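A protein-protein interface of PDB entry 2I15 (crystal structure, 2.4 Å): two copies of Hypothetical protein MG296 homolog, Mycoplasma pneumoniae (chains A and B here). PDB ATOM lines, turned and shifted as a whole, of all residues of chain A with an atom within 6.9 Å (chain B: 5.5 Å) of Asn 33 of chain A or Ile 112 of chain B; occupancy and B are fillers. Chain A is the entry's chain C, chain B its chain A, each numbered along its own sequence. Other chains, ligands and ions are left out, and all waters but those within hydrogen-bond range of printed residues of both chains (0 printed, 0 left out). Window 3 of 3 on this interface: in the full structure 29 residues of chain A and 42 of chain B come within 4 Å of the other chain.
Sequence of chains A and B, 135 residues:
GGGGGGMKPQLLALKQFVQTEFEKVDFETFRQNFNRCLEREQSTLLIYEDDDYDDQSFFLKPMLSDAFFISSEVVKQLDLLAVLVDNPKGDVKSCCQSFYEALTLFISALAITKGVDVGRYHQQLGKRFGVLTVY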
ATOM      1  N   PHE A  27      35.501  14.314  10.393  1.00  0.00           N
ATOM      2  CA  PHE A  27      34.471  13.585   9.661  1.00  0.00           C
ATOM      3  C   PHE A  27      34.238  12.134  10.052  1.00  0.00           C
ATOM      4  O   PHE A  27      33.115  11.740  10.349  1.00  0.00           O
ATOM      5  CB  PHE A  27      34.739  13.614   8.162  1.00  0.00           C
ATOM      6  CG  PHE A  27      33.708  12.876   7.377  1.00  0.00           C
ATOM      7  CD1 PHE A  27      32.493  13.483   7.075  1.00  0.00           C
ATOM      8  CD2 PHE A  27      33.914  11.549   7.010  1.00  0.00           C
ATOM      9  CE1 PHE A  27      31.492  12.780   6.424  1.00  0.00           C
ATOM     10  CE2 PHE A  27      32.915  10.836   6.359  1.00  0.00           C
ATOM     11  CZ  PHE A  27      31.701  11.454   6.064  1.00  0.00           C
ATOM     12  N   GLU A  28      35.294  11.333  10.013  1.00  0.00           N
ATOM     13  CA  GLU A  28      35.178   9.927  10.356  1.00  0.00           C
ATOM     14  C   GLU A  28      34.549   9.731  11.745  1.00  0.00           C
ATOM     15  O   GLU A  28      33.709   8.858  11.948  1.00  0.00           O
ATOM     16  CB  GLU A  28      36.548   9.264  10.260  1.00  0.00           C
ATOM     17  CG  GLU A  28      36.630   8.120   9.242  1.00  0.00           C
ATOM     18  CD  GLU A  28      36.021   8.451   7.881  1.00  0.00           C
ATOM     19  OE1 GLU A  28      36.446   9.445   7.253  1.00  0.00           O
ATOM     20  OE2 GLU A  28      35.126   7.699   7.431  1.00  0.00           O
ATOM     21  N   THR A  29      34.928  10.576  12.692  1.00  0.00           N
ATOM     22  CA  THR A  29      34.377  10.504  14.035  1.00  0.00           C
ATOM     23  C   THR A  29      32.924  10.934  13.968  1.00  0.00           C
ATOM     24  O   THR A  29      32.042  10.280  14.541  1.00  0.00           O
ATOM     25  CB  THR A  29      35.118  11.437  14.998  1.00  0.00           C
ATOM     26  OG1 THR A  29      36.520  11.138  14.956  1.00  0.00           O
ATOM     27  CG2 THR A  29      34.604  11.248  16.420  1.00  0.00           C
ATOM     28  N   PHE A  30      32.676  12.039  13.266  1.00  0.00           N
ATOM     29  CA  PHE A  30      31.316  12.540  13.125  1.00  0.00           C
ATOM     30  C   PHE A  30      30.412  11.466  12.542  1.00  0.00           C
ATOM     31  O   PHE A  30      29.392  11.122  13.114  1.00  0.00           O
ATOM     32  CB  PHE A  30      31.257  13.753  12.188  1.00  0.00           C
ATOM     33  CG  PHE A  30      29.851  14.220  11.903  1.00  0.00           C
ATOM     34  CD1 PHE A  30      29.106  14.859  12.889  1.00  0.00           C
ATOM     35  CD2 PHE A  30      29.254  13.958  10.677  1.00  0.00           C
ATOM     36  CE1 PHE A  30      27.776  15.233  12.663  1.00  0.00           C
ATOM     37  CE2 PHE A  30      27.926  14.321  10.434  1.00  0.00           C
ATOM     38  CZ  PHE A  30      27.186  14.960  11.433  1.00  0.00           C
ATOM     39  N   ARG A  31      30.810  10.967  11.379  1.00  0.00           N
ATOM     40  CA  ARG A  31      30.072   9.961  10.657  1.00  0.00           C
ATOM     41  C   ARG A  31      29.708   8.738  11.504  1.00  0.00           C
ATOM     42  O   ARG A  31      28.605   8.201  11.399  1.00  0.00           O
ATOM     43  CB  ARG A  31      30.867   9.544   9.419  1.00  0.00           C
ATOM     44  CG  ARG A  31      30.203   8.417   8.628  1.00  0.00           C
ATOM     45  CD  ARG A  31      31.095   7.179   8.637  1.00  0.00           C
ATOM     46  NE  ARG A  31      32.105   7.228   7.588  1.00  0.00           N
ATOM     47  CZ  ARG A  31      31.841   7.039   6.298  1.00  0.00           C
ATOM     48  NH1 ARG A  31      30.608   6.782   5.893  1.00  0.00           N
ATOM     49  NH2 ARG A  31      32.811   7.121   5.401  1.00  0.00           N
ATOM     50  N   GLN A  32      30.638   8.287  12.335  1.00  0.00           N
ATOM     51  CA  GLN A  32      30.388   7.132  13.200  1.00  0.00           C
ATOM     52  C   GLN A  32      29.327   7.525  14.213  1.00  0.00           C
ATOM     53  O   GLN A  32      28.432   6.738  14.498  1.00  0.00           O
ATOM     54  CB  GLN A  32      31.645   6.705  13.961  1.00  0.00           C
ATOM     55  CG  GLN A  32      32.811   6.302  13.099  1.00  0.00           C
ATOM     56  CD  GLN A  32      34.040   5.992  13.934  1.00  0.00           C
ATOM     57  OE1 GLN A  32      34.334   6.685  14.910  1.00  0.00           O
ATOM     58  NE2 GLN A  32      34.766   4.957  13.550  1.00  0.00           N
ATOM     59  N   ASN A  33      29.445   8.736  14.761  1.00  0.00           N
ATOM     60  CA  ASN A  33      28.486   9.259  15.743  1.00  0.00           C
ATOM     61  C   ASN A  33      27.111   9.505  15.146  1.00  0.00           C
ATOM     62  O   ASN A  33      26.101   9.263  15.801  1.00  0.00           O
ATOM     63  CB  ASN A  33      28.969  10.575  16.354  1.00  0.00           C
ATOM     64  CG  ASN A  33      30.096  10.387  17.332  1.00  0.00           C
ATOM     65  OD1 ASN A  33      30.340   9.288  17.815  1.00  0.00           O
ATOM     66  ND2 ASN A  33      30.782  11.463  17.641  1.00  0.00           N
ATOM     67  N   PHE A  34      27.067  10.037  13.930  1.00  0.00           N
ATOM     68  CA  PHE A  34      25.787  10.269  13.277  1.00  0.00           C
ATOM     69  C   PHE A  34      25.130   8.922  13.012  1.00  0.00           C
ATOM     70  O   PHE A  34      23.931   8.760  13.223  1.00  0.00           O
ATOM     71  CB  PHE A  34      25.949  10.964  11.935  1.00  0.00           C
ATOM     72  CG  PHE A  34      24.664  11.078  11.167  1.00  0.00           C
ATOM     73  CD1 PHE A  34      23.708  12.034  11.514  1.00  0.00           C
ATOM     74  CD2 PHE A  34      24.396  10.220  10.111  1.00  0.00           C
ATOM     75  CE1 PHE A  34      22.500  12.133  10.809  1.00  0.00           C
ATOM     76  CE2 PHE A  34      23.184  10.318   9.403  1.00  0.00           C
ATOM     77  CZ  PHE A  34      22.242  11.278   9.763  1.00  0.00           C
ATOM     78  N   ASN A  35      25.923   7.969  12.531  1.00  0.00           N
ATOM     79  CA  ASN A  35      25.414   6.642  12.240  1.00  0.00           C
ATOM     80  C   ASN A  35      24.865   5.951  13.485  1.00  0.00           C
ATOM     81  O   ASN A  35      23.827   5.292  13.416  1.00  0.00           O
ATOM     82  CB  ASN A  35      26.509   5.777  11.629  1.00  0.00           C
ATOM     83  CG  ASN A  35      26.656   5.989  10.140  1.00  0.00           C
ATOM     84  OD1 ASN A  35      25.918   6.759   9.528  1.00  0.00           O
ATOM     85  ND2 ASN A  35      27.610   5.299   9.546  1.00  0.00           N
ATOM     86  N   ARG A  36      25.569   6.080  14.607  1.00  0.00           N
ATOM     87  CA  ARG A  36      25.130   5.463  15.861  1.00  0.00           C
ATOM     88  C   ARG A  36      23.828   6.071  16.359  1.00  0.00           C
ATOM     89  O   ARG A  36      22.949   5.344  16.799  1.00  0.00           O
ATOM     90  CB  ARG A  36      26.209   5.585  16.943  1.00  0.00           C
ATOM     91  CG  ARG A  36      27.197   4.425  16.955  1.00  0.00           C
ATOM     92  CD  ARG A  36      28.274   4.624  18.017  1.00  0.00           C
ATOM     93  NE  ARG A  36      29.615   4.595  17.434  1.00  0.00           N
ATOM     94  CZ  ARG A  36      30.741   4.664  18.137  1.00  0.00           C
ATOM     95  NH1 ARG A  36      30.697   4.766  19.460  1.00  0.00           N
ATOM     96  NH2 ARG A  36      31.913   4.626  17.516  1.00  0.00           N
ATOM     97  N   CYS A  37      23.707   7.395  16.290  1.00  0.00           N
ATOM     98  CA  CYS A  37      22.491   8.078  16.712  1.00  0.00           C
ATOM     99  C   CYS A  37      21.330   7.616  15.821  1.00  0.00           C
ATOM    100  O   CYS A  37      20.208   7.415  16.287  1.00  0.00           O
ATOM    101  CB  CYS A  37      22.653   9.590  16.574  1.00  0.00           C
ATOM    102  SG  CYS A  37      23.900  10.342  17.631  1.00  0.00           S
ATOM    103  N   LEU A  38      21.622   7.440  14.536  1.00  0.00           N
ATOM    104  CA  LEU A  38      20.629   7.017  13.568  1.00  0.00           C
ATOM    105  C   LEU A  38      20.061   5.635  13.858  1.00  0.00           C
ATOM    106  O   LEU A  38      18.841   5.460  13.881  1.00  0.00           O
ATOM    107  CB  LEU A  38      21.223   7.028  12.161  1.00  0.00           C
ATOM    108  CG  LEU A  38      20.445   7.775  11.076  1.00  0.00           C
ATOM    109  CD1 LEU A  38      20.597   7.019   9.762  1.00  0.00           C
ATOM    110  CD2 LEU A  38      18.963   7.917  11.423  1.00  0.00           C
ATOM    111  N   ILE B 107      22.436  17.380  14.464  1.00  0.00           N
ATOM    112  CA  ILE B 107      22.901  18.284  15.508  1.00  0.00           C
ATOM    113  C   ILE B 107      23.402  17.601  16.785  1.00  0.00           C
ATOM    114  O   ILE B 107      24.346  18.089  17.414  1.00  0.00           O
ATOM    115  CB  ILE B 107      21.793  19.283  15.818  1.00  0.00           C
ATOM    116  CG1 ILE B 107      21.537  20.120  14.553  1.00  0.00           C
ATOM    117  CG2 ILE B 107      22.188  20.184  16.998  1.00  0.00           C
ATOM    118  CD1 ILE B 107      20.327  20.978  14.632  1.00  0.00           C
ATOM    119  N   SER B 108      22.783  16.482  17.170  1.00  0.00           N
ATOM    120  CA  SER B 108      23.202  15.750  18.372  1.00  0.00           C
ATOM    121  C   SER B 108      24.561  15.112  18.125  1.00  0.00           C
ATOM    122  O   SER B 108      25.433  15.140  18.989  1.00  0.00           O
ATOM    123  CB  SER B 108      22.198  14.651  18.733  1.00  0.00           C
ATOM    124  OG  SER B 108      20.969  15.198  19.166  1.00  0.00           O
ATOM    125  N   ALA B 109      24.733  14.526  16.940  1.00  0.00           N
ATOM    126  CA  ALA B 109      25.996  13.892  16.562  1.00  0.00           C
ATOM    127  C   ALA B 109      27.112  14.927  16.674  1.00  0.00           C
ATOM    128  O   ALA B 109      28.179  14.669  17.244  1.00  0.00           O
ATOM    129  CB  ALA B 109      25.919  13.381  15.147  1.00  0.00           C
ATOM    130  N   LEU B 110      26.857  16.099  16.107  1.00  0.00           N
ATOM    131  CA  LEU B 110      27.809  17.200  16.151  1.00  0.00           C
ATOM    132  C   LEU B 110      28.274  17.358  17.598  1.00  0.00           C
ATOM    133  O   LEU B 110      29.471  17.421  17.890  1.00  0.00           O
ATOM    134  CB  LEU B 110      27.125  18.493  15.691  1.00  0.00           C
ATOM    135  CG  LEU B 110      26.811  18.690  14.210  1.00  0.00           C
ATOM    136  CD1 LEU B 110      26.053  19.987  14.028  1.00  0.00           C
ATOM    137  CD2 LEU B 110      28.106  18.713  13.407  1.00  0.00           C
ATOM    138  N   ALA B 111      27.294  17.426  18.496  1.00  0.00           N
ATOM    139  CA  ALA B 111      27.539  17.576  19.921  1.00  0.00           C
ATOM    140  C   ALA B 111      28.337  16.409  20.465  1.00  0.00           C
ATOM    141  O   ALA B 111      29.304  16.608  21.199  1.00  0.00           O
ATOM    142  CB  ALA B 111      26.218  17.706  20.667  1.00  0.00           C
ATOM    143  N   ILE B 112      27.932  15.189  20.117  1.00  0.00           N
ATOM    144  CA  ILE B 112      28.645  14.007  20.593  1.00  0.00           C
ATOM    145  C   ILE B 112      30.094  14.144  20.136  1.00  0.00           C
ATOM    146  O   ILE B 112      31.045  13.943  20.902  1.00  0.00           O
ATOM    147  CB  ILE B 112      28.078  12.703  19.982  1.00  0.00           C
ATOM    148  CG1 ILE B 112      26.569  12.625  20.191  1.00  0.00           C
ATOM    149  CG2 ILE B 112      28.733  11.494  20.637  1.00  0.00           C
ATOM    150  CD1 ILE B 112      26.171  12.492  21.623  1.00  0.00           C
ATOM    151  N   THR B 113      30.236  14.522  18.873  1.00  0.00           N
ATOM    152  CA  THR B 113      31.533  14.675  18.250  1.00  0.00           C
ATOM    153  C   THR B 113      32.422  15.759  18.856  1.00  0.00           C
ATOM    154  O   THR B 113      33.631  15.570  18.967  1.00  0.00           O
ATOM    155  CB  THR B 113      31.362  14.907  16.733  1.00  0.00           C
ATOM    156  OG1 THR B 113      30.435  13.938  16.232  1.00  0.00           O
ATOM    157  CG2 THR B 113      32.683  14.725  16.001  1.00  0.00           C
ATOM    158  N   LYS B 114      31.862  16.896  19.245  1.00  0.00           N
ATOM    159  CA  LYS B 114      32.733  17.905  19.833  1.00  0.00           C
ATOM    160  C   LYS B 114      32.834  17.814  21.346  1.00  0.00           C
ATOM    161  O   LYS B 114      33.345  18.721  22.005  1.00  0.00           O
ATOM    162  CB  LYS B 114      32.340  19.324  19.409  1.00  0.00           C
ATOM    163  CG  LYS B 114      30.884  19.699  19.477  1.00  0.00           C
ATOM    164  CD  LYS B 114      30.760  21.225  19.458  1.00  0.00           C
ATOM    165  CE  LYS B 114      31.599  21.865  18.357  1.00  0.00           C
ATOM    166  NZ  LYS B 114      31.730  23.355  18.539  1.00  0.00           N
ATOM    167  N   GLY B 115      32.372  16.696  21.889  1.00  0.00           N
ATOM    168  CA  GLY B 115      32.433  16.492  23.323  1.00  0.00           C
ATOM    169  C   GLY B 115      31.637  17.522  24.085  1.00  0.00           C
ATOM    170  O   GLY B 115      32.020  17.949  25.168  1.00  0.00           O
ATOM    171  N   VAL B 116      30.519  17.926  23.502  1.00  0.00           N
ATOM    172  CA  VAL B 116      29.656  18.910  24.125  1.00  0.00           C
ATOM    173  C   VAL B 116      28.415  18.249  24.678  1.00  0.00           C
ATOM    174  O   VAL B 116      27.993  17.198  24.201  1.00  0.00           O
ATOM    175  CB  VAL B 116      29.255  20.003  23.109  1.00  0.00           C
ATOM    176  CG1 VAL B 116      28.089  20.833  23.618  1.00  0.00           C
ATOM    177  CG2 VAL B 116      30.443  20.899  22.848  1.00  0.00           C
ATOM    178  N   VAL B 118      25.073  17.229  24.737  1.00  0.00           N
ATOM    179  CA  VAL B 118      23.940  17.275  23.829  1.00  0.00           C
ATOM    180  C   VAL B 118      22.937  17.949  24.762  1.00  0.00           C
ATOM    181  O   VAL B 118      23.119  17.931  25.981  1.00  0.00           O
ATOM    182  CB  VAL B 118      23.443  15.864  23.460  1.00  0.00           C
ATOM    183  CG1 VAL B 118      22.243  15.969  22.575  1.00  0.00           C
ATOM    184  CG2 VAL B 118      24.538  15.090  22.745  1.00  0.00           C
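The backbone carbonyl oxygen of Ala 109 of chain B lies within hydrogen-bond range of the side-chain hydroxyl of Thr 113 of chain B (2.6 Å). The side-chain sulfur (SG) of Cys 37 of chain A sits at hydrogen-bond distance from the backbone carbonyl oxygen (O) of Asn 33 of chain A.
Of the 12 printed residues of chain A, 4 touch a printed residue of chain B. Of the 11 printed residues of chain B, 4 touch a printed residue of chain A.
The side-chain hydroxyl (OG1) of Thr 113 of chain B sits at hydrogen-bond distance from the side-chain amide nitrogen (ND2) of Asn 33 of chain A, at 2.9 Å.
Of the printed residues of chain B, Thr 29 of chain A touches Thr 113. Of the printed residues of chain B, Phe 30 of chain A touches Ala 109, Leu 110 and Thr 113. Of chain B, only Ile 112 and Thr 113 come within 4 Å of Asn 33 of chain A. Of the printed residues of chain A, Ala 109 of chain B touches Phe 30 (3.6 Å) and Phe 34 (3.6 Å). Ile 112 of chain B touches just one residue of chain A: Asn 33 (3.6 Å). Printed residues of chain A within 4 Å of Thr 113 of chain B: Thr 29, Phe 30 and Asn 33. The nearest residue of chain B that does not touch Asn 33 of chain A is Ala 109 of chain B (4.1 Å). The nearest residue of chain A that does not touch Ile 112 of chain B is Cys 37 of chain A (4.3 Å).
No position is printed for both chains. Of the 7 pairs that touch across the chains among the printed residues, none has its exchanged pair printed and touching as well.
Among the printed residues, merely in contact across the chains: Phe 30 of chain A with Thr 113 of chain B (3.5 Å), Phe 30 of chain A with Leu 110 of chain B (3.6 Å), Phe 30 of chain A with Ala 109 of chain B (3.6 Å), Asn 33 of chain A with Ile 112 of chain B (3.6 Å), Phe 34 of chain A with Ala 109 of chain B (3.6 Å) and Thr 29 of chain A with Thr 113 of chain B (3.99 Å).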
